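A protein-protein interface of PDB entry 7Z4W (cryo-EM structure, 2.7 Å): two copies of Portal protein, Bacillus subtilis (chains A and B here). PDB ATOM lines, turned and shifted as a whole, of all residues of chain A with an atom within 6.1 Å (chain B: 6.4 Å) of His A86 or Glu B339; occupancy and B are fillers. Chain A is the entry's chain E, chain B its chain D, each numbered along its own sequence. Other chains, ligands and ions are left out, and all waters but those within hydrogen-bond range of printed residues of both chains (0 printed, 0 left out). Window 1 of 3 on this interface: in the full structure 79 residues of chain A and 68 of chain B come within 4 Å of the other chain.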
ATOM      1  N   TYR A  52      25.492 -29.295 -16.354  1.00  0.00           N
ATOM      2  CA  TYR A  52      24.371 -28.697 -15.642  1.00  0.00           C
ATOM      3  C   TYR A  52      23.141 -29.594 -15.635  1.00  0.00           C
ATOM      4  O   TYR A  52      22.279 -29.426 -14.768  1.00  0.00           O
ATOM      5  CB  TYR A  52      24.027 -27.339 -16.248  1.00  0.00           C
ATOM      6  CG  TYR A  52      24.846 -26.195 -15.694  1.00  0.00           C
ATOM      7  CD1 TYR A  52      26.220 -26.131 -15.903  1.00  0.00           C
ATOM      8  CD2 TYR A  52      24.245 -25.172 -14.975  1.00  0.00           C
ATOM      9  CE1 TYR A  52      26.965 -25.094 -15.413  1.00  0.00           C
ATOM     10  CE2 TYR A  52      24.990 -24.123 -14.476  1.00  0.00           C
ATOM     11  CZ  TYR A  52      26.349 -24.094 -14.698  1.00  0.00           C
ATOM     12  OH  TYR A  52      27.095 -23.060 -14.205  1.00  0.00           O
ATOM     13  N   CYS A  55      23.344 -31.755 -12.447  1.00  0.00           N
ATOM     14  CA  CYS A  55      23.491 -30.836 -11.302  1.00  0.00           C
ATOM     15  C   CYS A  55      24.928 -30.759 -10.775  1.00  0.00           C
ATOM     16  O   CYS A  55      25.201 -30.906  -9.584  1.00  0.00           O
ATOM     17  CB  CYS A  55      22.484 -31.157 -10.179  1.00  0.00           C
ATOM     18  SG  CYS A  55      22.562 -32.738  -9.289  1.00  0.00           S
ATOM     19  N   ASN A  57      27.147 -27.773 -11.221  1.00  0.00           N
ATOM     20  CA  ASN A  57      27.228 -26.406 -11.701  1.00  0.00           C
ATOM     21  C   ASN A  57      28.579 -25.798 -11.328  1.00  0.00           C
ATOM     22  O   ASN A  57      29.425 -26.438 -10.705  1.00  0.00           O
ATOM     23  CB  ASN A  57      26.060 -25.592 -11.149  1.00  0.00           C
ATOM     24  CG  ASN A  57      24.714 -26.258 -11.392  1.00  0.00           C
ATOM     25  OD1 ASN A  57      24.617 -27.250 -12.108  1.00  0.00           O
ATOM     26  ND2 ASN A  57      23.669 -25.713 -10.791  1.00  0.00           N
ATOM     27  N   THR A  84      25.821 -25.765  -3.036  1.00  0.00           N
ATOM     28  CA  THR A  84      24.549 -26.383  -3.395  1.00  0.00           C
ATOM     29  C   THR A  84      24.202 -26.054  -4.843  1.00  0.00           C
ATOM     30  O   THR A  84      24.045 -24.882  -5.196  1.00  0.00           O
ATOM     31  CB  THR A  84      23.436 -25.915  -2.455  1.00  0.00           C
ATOM     32  OG1 THR A  84      23.698 -26.399  -1.134  1.00  0.00           O
ATOM     33  CG2 THR A  84      22.083 -26.432  -2.913  1.00  0.00           C
ATOM     34  N   SER A  85      24.089 -27.091  -5.672  1.00  0.00           N
ATOM     35  CA  SER A  85      23.668 -26.951  -7.061  1.00  0.00           C
ATOM     36  C   SER A  85      22.170 -27.203  -7.175  1.00  0.00           C
ATOM     37  O   SER A  85      21.648 -28.150  -6.581  1.00  0.00           O
ATOM     38  CB  SER A  85      24.425 -27.924  -7.965  1.00  0.00           C
ATOM     39  OG  SER A  85      25.817 -27.878  -7.737  1.00  0.00           O
ATOM     40  N   HIS A  86      21.484 -26.360  -7.934  1.00  0.00           N
ATOM     41  CA  HIS A  86      20.059 -26.516  -8.174  1.00  0.00           C
ATOM     42  C   HIS A  86      19.815 -27.073  -9.572  1.00  0.00           C
ATOM     43  O   HIS A  86      20.590 -26.838 -10.500  1.00  0.00           O
ATOM     44  CB  HIS A  86      19.332 -25.185  -7.979  1.00  0.00           C
ATOM     45  CG  HIS A  86      19.345 -24.702  -6.562  1.00  0.00           C
ATOM     46  ND1 HIS A  86      20.396 -23.986  -6.029  1.00  0.00           N
ATOM     47  CD2 HIS A  86      18.447 -24.850  -5.560  1.00  0.00           C
ATOM     48  CE1 HIS A  86      20.142 -23.708  -4.764  1.00  0.00           C
ATOM     49  NE2 HIS A  86      18.964 -24.218  -4.456  1.00  0.00           N
ATOM     50  N   ALA A  87      18.720 -27.817  -9.710  1.00  0.00           N
ATOM     51  CA  ALA A  87      18.453 -28.662 -10.874  1.00  0.00           C
ATOM     52  C   ALA A  87      17.421 -28.061 -11.821  1.00  0.00           C
ATOM     53  O   ALA A  87      16.535 -28.774 -12.298  1.00  0.00           O
ATOM     54  CB  ALA A  87      18.016 -30.051 -10.421  1.00  0.00           C
ATOM     55  N   TRP A  88      17.495 -26.753 -12.081  1.00  0.00           N
ATOM     56  CA  TRP A  88      16.529 -26.087 -12.953  1.00  0.00           C
ATOM     57  C   TRP A  88      16.640 -26.566 -14.401  1.00  0.00           C
ATOM     58  O   TRP A  88      15.619 -26.767 -15.077  1.00  0.00           O
ATOM     59  CB  TRP A  88      16.732 -24.573 -12.880  1.00  0.00           C
ATOM     60  CG  TRP A  88      16.563 -23.974 -11.508  1.00  0.00           C
ATOM     61  CD1 TRP A  88      17.556 -23.533 -10.680  1.00  0.00           C
ATOM     62  CD2 TRP A  88      15.331 -23.720 -10.820  1.00  0.00           C
ATOM     63  NE1 TRP A  88      17.022 -23.037  -9.518  1.00  0.00           N
ATOM     64  CE2 TRP A  88      15.659 -23.139  -9.577  1.00  0.00           C
ATOM     65  CE3 TRP A  88      13.985 -23.935 -11.130  1.00  0.00           C
ATOM     66  CZ2 TRP A  88      14.689 -22.770  -8.647  1.00  0.00           C
ATOM     67  CZ3 TRP A  88      13.024 -23.567 -10.205  1.00  0.00           C
ATOM     68  CH2 TRP A  88      13.381 -22.991  -8.978  1.00  0.00           C
ATOM     69  N   HIS A  89      17.873 -26.771 -14.881  1.00  0.00           N
ATOM     70  CA  HIS A  89      18.120 -27.087 -16.286  1.00  0.00           C
ATOM     71  C   HIS A  89      17.579 -28.463 -16.663  1.00  0.00           C
ATOM     72  O   HIS A  89      17.008 -28.633 -17.747  1.00  0.00           O
ATOM     73  CB  HIS A  89      19.621 -26.992 -16.572  1.00  0.00           C
ATOM     74  CG  HIS A  89      20.005 -27.367 -17.971  1.00  0.00           C
ATOM     75  ND1 HIS A  89      19.633 -26.627 -19.071  1.00  0.00           N
ATOM     76  CD2 HIS A  89      20.735 -28.402 -18.446  1.00  0.00           C
ATOM     77  CE1 HIS A  89      20.114 -27.192 -20.163  1.00  0.00           C
ATOM     78  NE2 HIS A  89      20.787 -28.270 -19.811  1.00  0.00           N
ATOM     79  N   ILE A 264      20.999 -19.010 -12.827  1.00  0.00           N
ATOM     80  CA  ILE A 264      21.269 -20.212 -12.040  1.00  0.00           C
ATOM     81  C   ILE A 264      22.491 -20.004 -11.150  1.00  0.00           C
ATOM     82  O   ILE A 264      22.496 -20.398  -9.972  1.00  0.00           O
ATOM     83  CB  ILE A 264      21.440 -21.427 -12.977  1.00  0.00           C
ATOM     84  CG1 ILE A 264      20.145 -21.698 -13.744  1.00  0.00           C
ATOM     85  CG2 ILE A 264      21.870 -22.676 -12.211  1.00  0.00           C
ATOM     86  CD1 ILE A 264      20.194 -22.921 -14.637  1.00  0.00           C
ATOM     87  N   TYR A 267      21.512 -17.664  -8.224  1.00  0.00           N
ATOM     88  CA  TYR A 267      20.707 -18.441  -7.280  1.00  0.00           C
ATOM     89  C   TYR A 267      21.580 -19.322  -6.387  1.00  0.00           C
ATOM     90  O   TYR A 267      21.442 -19.308  -5.148  1.00  0.00           O
ATOM     91  CB  TYR A 267      19.707 -19.291  -8.073  1.00  0.00           C
ATOM     92  CG  TYR A 267      18.462 -19.699  -7.328  1.00  0.00           C
ATOM     93  CD1 TYR A 267      18.466 -20.800  -6.481  1.00  0.00           C
ATOM     94  CD2 TYR A 267      17.275 -18.998  -7.488  1.00  0.00           C
ATOM     95  CE1 TYR A 267      17.332 -21.178  -5.801  1.00  0.00           C
ATOM     96  CE2 TYR A 267      16.133 -19.368  -6.809  1.00  0.00           C
ATOM     97  CZ  TYR A 267      16.169 -20.459  -5.968  1.00  0.00           C
ATOM     98  OH  TYR A 267      15.041 -20.839  -5.290  1.00  0.00           O
ATOM     99  N   ASP A 268      22.512 -20.062  -7.004  1.00  0.00           N
ATOM    100  CA  ASP A 268      23.393 -20.966  -6.267  1.00  0.00           C
ATOM    101  C   ASP A 268      24.293 -20.212  -5.291  1.00  0.00           C
ATOM    102  O   ASP A 268      24.446 -20.629  -4.133  1.00  0.00           O
ATOM    103  CB  ASP A 268      24.245 -21.778  -7.241  1.00  0.00           C
ATOM    104  CG  ASP A 268      23.457 -22.850  -7.965  1.00  0.00           C
ATOM    105  OD1 ASP A 268      22.263 -23.034  -7.660  1.00  0.00           O
ATOM    106  OD2 ASP A 268      24.036 -23.512  -8.846  1.00  0.00           O
ATOM    107  N   THR A 271      22.207 -18.730  -2.184  1.00  0.00           N
ATOM    108  CA  THR A 271      21.774 -19.744  -1.220  1.00  0.00           C
ATOM    109  C   THR A 271      22.950 -20.394  -0.488  1.00  0.00           C
ATOM    110  O   THR A 271      22.838 -20.693   0.712  1.00  0.00           O
ATOM    111  CB  THR A 271      20.907 -20.808  -1.902  1.00  0.00           C
ATOM    112  OG1 THR A 271      21.598 -21.369  -3.021  1.00  0.00           O
ATOM    113  CG2 THR A 271      19.598 -20.209  -2.371  1.00  0.00           C
ATOM    114  N   LEU A 333      15.761 -13.732  -4.479  1.00  0.00           N
ATOM    115  CA  LEU A 333      15.530 -15.044  -5.076  1.00  0.00           C
ATOM    116  C   LEU A 333      14.138 -15.161  -5.685  1.00  0.00           C
ATOM    117  O   LEU A 333      13.963 -15.898  -6.663  1.00  0.00           O
ATOM    118  CB  LEU A 333      15.745 -16.154  -4.046  1.00  0.00           C
ATOM    119  CG  LEU A 333      17.174 -16.412  -3.553  1.00  0.00           C
ATOM    120  CD1 LEU A 333      17.164 -17.270  -2.300  1.00  0.00           C
ATOM    121  CD2 LEU A 333      18.066 -17.007  -4.622  1.00  0.00           C
ATOM    122  N   GLN A 337      13.711 -16.213  -9.578  1.00  0.00           N
ATOM    123  CA  GLN A 337      12.900 -17.350 -10.013  1.00  0.00           C
ATOM    124  C   GLN A 337      11.858 -16.941 -11.055  1.00  0.00           C
ATOM    125  O   GLN A 337      11.634 -17.669 -12.042  1.00  0.00           O
ATOM    126  CB  GLN A 337      12.225 -17.999  -8.807  1.00  0.00           C
ATOM    127  CG  GLN A 337      11.512 -19.294  -9.129  1.00  0.00           C
ATOM    128  CD  GLN A 337      10.865 -19.926  -7.921  1.00  0.00           C
ATOM    129  OE1 GLN A 337      11.457 -19.987  -6.846  1.00  0.00           O
ATOM    130  NE2 GLN A 337       9.640 -20.402  -8.092  1.00  0.00           N
ATOM    131  N   PHE B 259      19.712 -35.928  -7.419  1.00  0.00           N
ATOM    132  CA  PHE B 259      19.230 -34.620  -7.832  1.00  0.00           C
ATOM    133  C   PHE B 259      18.697 -33.761  -6.688  1.00  0.00           C
ATOM    134  O   PHE B 259      18.415 -32.582  -6.914  1.00  0.00           O
ATOM    135  CB  PHE B 259      18.165 -34.786  -8.920  1.00  0.00           C
ATOM    136  CG  PHE B 259      18.659 -35.542 -10.121  1.00  0.00           C
ATOM    137  CD1 PHE B 259      19.488 -34.927 -11.049  1.00  0.00           C
ATOM    138  CD2 PHE B 259      18.320 -36.871 -10.311  1.00  0.00           C
ATOM    139  CE1 PHE B 259      19.958 -35.619 -12.144  1.00  0.00           C
ATOM    140  CE2 PHE B 259      18.785 -37.568 -11.406  1.00  0.00           C
ATOM    141  CZ  PHE B 259      19.607 -36.939 -12.324  1.00  0.00           C
ATOM    142  N   TYR B 260      18.551 -34.304  -5.470  1.00  0.00           N
ATOM    143  CA  TYR B 260      18.064 -33.484  -4.364  1.00  0.00           C
ATOM    144  C   TYR B 260      18.720 -33.796  -3.016  1.00  0.00           C
ATOM    145  O   TYR B 260      18.105 -33.539  -1.976  1.00  0.00           O
ATOM    146  CB  TYR B 260      16.533 -33.604  -4.240  1.00  0.00           C
ATOM    147  CG  TYR B 260      15.990 -35.018  -4.232  1.00  0.00           C
ATOM    148  CD1 TYR B 260      15.931 -35.753  -3.056  1.00  0.00           C
ATOM    149  CD2 TYR B 260      15.518 -35.609  -5.398  1.00  0.00           C
ATOM    150  CE1 TYR B 260      15.436 -37.036  -3.040  1.00  0.00           C
ATOM    151  CE2 TYR B 260      15.019 -36.896  -5.392  1.00  0.00           C
ATOM    152  CZ  TYR B 260      14.979 -37.602  -4.208  1.00  0.00           C
ATOM    153  OH  TYR B 260      14.484 -38.881  -4.186  1.00  0.00           O
ATOM    154  N   LEU B 263      19.567 -30.578  -0.599  1.00  0.00           N
ATOM    155  CA  LEU B 263      18.435 -29.945   0.069  1.00  0.00           C
ATOM    156  C   LEU B 263      18.021 -30.715   1.318  1.00  0.00           C
ATOM    157  O   LEU B 263      17.694 -30.110   2.348  1.00  0.00           O
ATOM    158  CB  LEU B 263      17.270 -29.822  -0.911  1.00  0.00           C
ATOM    159  CG  LEU B 263      17.572 -29.103  -2.227  1.00  0.00           C
ATOM    160  CD1 LEU B 263      16.458 -29.320  -3.236  1.00  0.00           C
ATOM    161  CD2 LEU B 263      17.799 -27.620  -1.999  1.00  0.00           C
ATOM    162  N   GLU B 334      10.892 -23.076   4.602  1.00  0.00           N
ATOM    163  CA  GLU B 334       9.782 -22.973   3.651  1.00  0.00           C
ATOM    164  C   GLU B 334      10.268 -23.007   2.202  1.00  0.00           C
ATOM    165  O   GLU B 334       9.701 -23.723   1.364  1.00  0.00           O
ATOM    166  CB  GLU B 334       8.985 -21.698   3.905  1.00  0.00           C
ATOM    167  CG  GLU B 334       7.995 -21.799   5.032  1.00  0.00           C
ATOM    168  CD  GLU B 334       7.481 -20.444   5.476  1.00  0.00           C
ATOM    169  OE1 GLU B 334       6.268 -20.329   5.755  1.00  0.00           O
ATOM    170  OE2 GLU B 334       8.289 -19.494   5.550  1.00  0.00           O
ATOM    171  N   ARG B 335      11.342 -22.270   1.901  1.00  0.00           N
ATOM    172  CA  ARG B 335      11.881 -22.251   0.544  1.00  0.00           C
ATOM    173  C   ARG B 335      12.521 -23.586   0.176  1.00  0.00           C
ATOM    174  O   ARG B 335      12.404 -24.035  -0.971  1.00  0.00           O
ATOM    175  CB  ARG B 335      12.887 -21.109   0.389  1.00  0.00           C
ATOM    176  CG  ARG B 335      13.298 -20.849  -1.058  1.00  0.00           C
ATOM    177  CD  ARG B 335      14.486 -19.906  -1.202  1.00  0.00           C
ATOM    178  NE  ARG B 335      15.458 -20.021  -0.118  1.00  0.00           N
ATOM    179  CZ  ARG B 335      16.437 -20.917  -0.079  1.00  0.00           C
ATOM    180  NH1 ARG B 335      16.579 -21.791  -1.063  1.00  0.00           N
ATOM    181  NH2 ARG B 335      17.270 -20.942   0.946  1.00  0.00           N
ATOM    182  N   ILE B 336      13.186 -24.239   1.137  1.00  0.00           N
ATOM    183  CA  ILE B 336      13.795 -25.540   0.855  1.00  0.00           C
ATOM    184  C   ILE B 336      12.722 -26.598   0.594  1.00  0.00           C
ATOM    185  O   ILE B 336      12.854 -27.418  -0.326  1.00  0.00           O
ATOM    186  CB  ILE B 336      14.748 -25.946   1.998  1.00  0.00           C
ATOM    187  CG1 ILE B 336      15.964 -25.020   2.027  1.00  0.00           C
ATOM    188  CG2 ILE B 336      15.227 -27.385   1.852  1.00  0.00           C
ATOM    189  CD1 ILE B 336      16.878 -25.252   3.205  1.00  0.00           C
ATOM    190  N   GLN B 337      11.623 -26.566   1.359  1.00  0.00           N
ATOM    191  CA  GLN B 337      10.527 -27.502   1.123  1.00  0.00           C
ATOM    192  C   GLN B 337       9.826 -27.237  -0.206  1.00  0.00           C
ATOM    193  O   GLN B 337       9.383 -28.185  -0.864  1.00  0.00           O
ATOM    194  CB  GLN B 337       9.524 -27.446   2.275  1.00  0.00           C
ATOM    195  CG  GLN B 337       8.501 -28.569   2.246  1.00  0.00           C
ATOM    196  CD  GLN B 337       7.419 -28.421   3.290  1.00  0.00           C
ATOM    197  OE1 GLN B 337       7.700 -28.310   4.482  1.00  0.00           O
ATOM    198  NE2 GLN B 337       6.171 -28.418   2.846  1.00  0.00           N
ATOM    199  N   ASP B 338       9.730 -25.972  -0.625  1.00  0.00           N
ATOM    200  CA  ASP B 338       9.195 -25.681  -1.953  1.00  0.00           C
ATOM    201  C   ASP B 338      10.114 -26.189  -3.062  1.00  0.00           C
ATOM    202  O   ASP B 338       9.636 -26.695  -4.082  1.00  0.00           O
ATOM    203  CB  ASP B 338       8.959 -24.183  -2.114  1.00  0.00           C
ATOM    204  CG  ASP B 338       7.571 -23.765  -1.696  1.00  0.00           C
ATOM    205  OD1 ASP B 338       6.721 -24.657  -1.496  1.00  0.00           O
ATOM    206  OD2 ASP B 338       7.329 -22.547  -1.564  1.00  0.00           O
ATOM    207  N   GLU B 339      11.432 -26.057  -2.886  1.00  0.00           N
ATOM    208  CA  GLU B 339      12.363 -26.486  -3.929  1.00  0.00           C
ATOM    209  C   GLU B 339      12.480 -28.004  -4.009  1.00  0.00           C
ATOM    210  O   GLU B 339      12.815 -28.540  -5.074  1.00  0.00           O
ATOM    211  CB  GLU B 339      13.743 -25.875  -3.694  1.00  0.00           C
ATOM    212  CG  GLU B 339      13.832 -24.395  -3.998  1.00  0.00           C
ATOM    213  CD  GLU B 339      14.964 -23.712  -3.258  1.00  0.00           C
ATOM    214  OE1 GLU B 339      15.659 -24.387  -2.473  1.00  0.00           O
ATOM    215  OE2 GLU B 339      15.158 -22.497  -3.457  1.00  0.00           O
ATOM    216  N   LEU B 340      12.217 -28.705  -2.903  1.00  0.00           N
ATOM    217  CA  LEU B 340      12.392 -30.154  -2.864  1.00  0.00           C
ATOM    218  C   LEU B 340      11.370 -30.876  -3.739  1.00  0.00           C
ATOM    219  O   LEU B 340      11.715 -31.839  -4.438  1.00  0.00           O
ATOM    220  CB  LEU B 340      12.301 -30.632  -1.417  1.00  0.00           C
ATOM    221  CG  LEU B 340      12.954 -31.944  -0.998  1.00  0.00           C
ATOM    222  CD1 LEU B 340      14.357 -32.069  -1.553  1.00  0.00           C
ATOM    223  CD2 LEU B 340      12.972 -32.032   0.513  1.00  0.00           C
ATOM    224  N   TYR B 341      10.115 -30.416  -3.723  1.00  0.00           N
ATOM    225  CA  TYR B 341       9.071 -31.021  -4.546  1.00  0.00           C
ATOM    226  C   TYR B 341       9.316 -30.789  -6.032  1.00  0.00           C
ATOM    227  O   TYR B 341       8.979 -31.646  -6.854  1.00  0.00           O
ATOM    228  CB  TYR B 341       7.703 -30.467  -4.151  1.00  0.00           C
ATOM    229  CG  TYR B 341       7.093 -31.108  -2.926  1.00  0.00           C
ATOM    230  CD1 TYR B 341       6.538 -32.379  -2.984  1.00  0.00           C
ATOM    231  CD2 TYR B 341       7.069 -30.435  -1.710  1.00  0.00           C
ATOM    232  CE1 TYR B 341       5.978 -32.965  -1.863  1.00  0.00           C
ATOM    233  CE2 TYR B 341       6.516 -31.012  -0.586  1.00  0.00           C
ATOM    234  CZ  TYR B 341       5.972 -32.274  -0.669  1.00  0.00           C
ATOM    235  OH  TYR B 341       5.419 -32.845   0.450  1.00  0.00           O
ATOM    236  N   LYS B 342       9.903 -29.647  -6.391  1.00  0.00           N
ATOM    237  CA  LYS B 342      10.226 -29.376  -7.786  1.00  0.00           C
ATOM    238  C   LYS B 342      11.441 -30.171  -8.245  1.00  0.00           C
ATOM    239  O   LYS B 342      11.473 -30.652  -9.382  1.00  0.00           O
ATOM    240  CB  LYS B 342      10.457 -27.880  -7.990  1.00  0.00           C
ATOM    241  CG  LYS B 342       9.188 -27.091  -8.223  1.00  0.00           C
ATOM    242  CD  LYS B 342       9.465 -25.611  -8.400  1.00  0.00           C
ATOM    243  CE  LYS B 342       8.173 -24.809  -8.367  1.00  0.00           C
ATOM    244  NZ  LYS B 342       8.405 -23.342  -8.405  1.00  0.00           N
ATOM    245  N   SER B 343      12.447 -30.322  -7.380  1.00  0.00           N
ATOM    246  CA  SER B 343      13.643 -31.060  -7.763  1.00  0.00           C
ATOM    247  C   SER B 343      13.413 -32.564  -7.795  1.00  0.00           C
ATOM    248  O   SER B 343      14.109 -33.271  -8.528  1.00  0.00           O
ATOM    249  CB  SER B 343      14.794 -30.732  -6.813  1.00  0.00           C
ATOM    250  OG  SER B 343      15.154 -29.369  -6.907  1.00  0.00           O
ATOM    251  N   ALA B 344      12.460 -33.074  -7.017  1.00  0.00           N
ATOM    252  CA  ALA B 344      12.174 -34.501  -7.030  1.00  0.00           C
ATOM    253  C   ALA B 344      11.109 -34.895  -8.044  1.00  0.00           C
ATOM    254  O   ALA B 344      10.978 -36.091  -8.329  1.00  0.00           O
ATOM    255  CB  ALA B 344      11.739 -34.966  -5.639  1.00  0.00           C
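The side-chain carboxylate of Glu B339 sits at hydrogen-bond distance from the side-chain hydroxyl of Tyr A267 (2.5 Å). NZ of Lys B342 lies close to NE2 of Gln A337, 3.2 Å away.
Position printed for both chains: 337.
His A86 touches just one residue of chain B: Glu B339. Of chain A, only His A86 and Tyr A267 come within 4 Å of Glu B339. Printed residues of chain B within 4 Å of Thr A271: Arg B335. Of the printed residues of chain B, Gln A337 touches Lys B342 (3.2 Å). Of the printed residues of chain B, Tyr A267 touches Glu B339. Of the printed residues of chain A, Lys B342 touches Gln A337 (3.2 Å). Of the printed residues of chain B, Leu A333 touches Arg B335. Trp A88 touches none of the printed residues of chain B. Leu B263 touches none of the printed residues of chain A. The nearest residue of chain B that does not touch His A86 is Leu B263 (4.4 Å). The nearest residue of chain A that does not touch Glu B339 is Trp A88 (5.0 Å).
Of the 14 printed residues of chain B, 3 touch a printed residue of chain A. Printed residues of chain A that touch a printed residue of chain B: His A86, Tyr A267, Thr A271, Leu A333 and Gln A337. Hydrophobic or aromatic side chains of chain A within 4 Å of the printed part of chain B: His A86, Tyr A267 and Leu A333. Among the printed residues, 5 pairs touch across the chains. Among the printed residues, no Asp or Glu carboxylate lies within 4 Å of a Lys or Arg side-chain nitrogen of the other chain.
Among the printed residues, merely in contact across the chains: His A86 with Glu B339 (3.9 Å), Thr A271 with Arg B335 (3.7 Å) and Leu A333 with Arg B335 (3.9 Å).
The guanidinium group (NH1) of Arg B335 is in salt-bridge range of the side-chain carboxylate (OE2) of Glu B339, at 2.9 Å. The backbone carbonyl oxygen of Glu B339 is in hydrogen-bond range of the side-chain hydroxyl of Ser B343 (3.1 Å). The side-chain amide nitrogen (ND2) of Asn A57 is in hydrogen-bond range of the backbone carbonyl oxygen (O) of His A86, at 3.3 Å. ND1 of His A86 is in hydrogen-bond range of OD1 of Asp A268 (2.7 Å). The side-chain hydroxyl of Thr A271 is in hydrogen-bond range of the backbone carbonyl oxygen of Tyr A267 (3.0 Å). The backbone carbonyl oxygen (O) of Asp A268 sits at hydrogen-bond distance from the side-chain hydroxyl (OG1) of Thr A271, at 3.1 Å.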
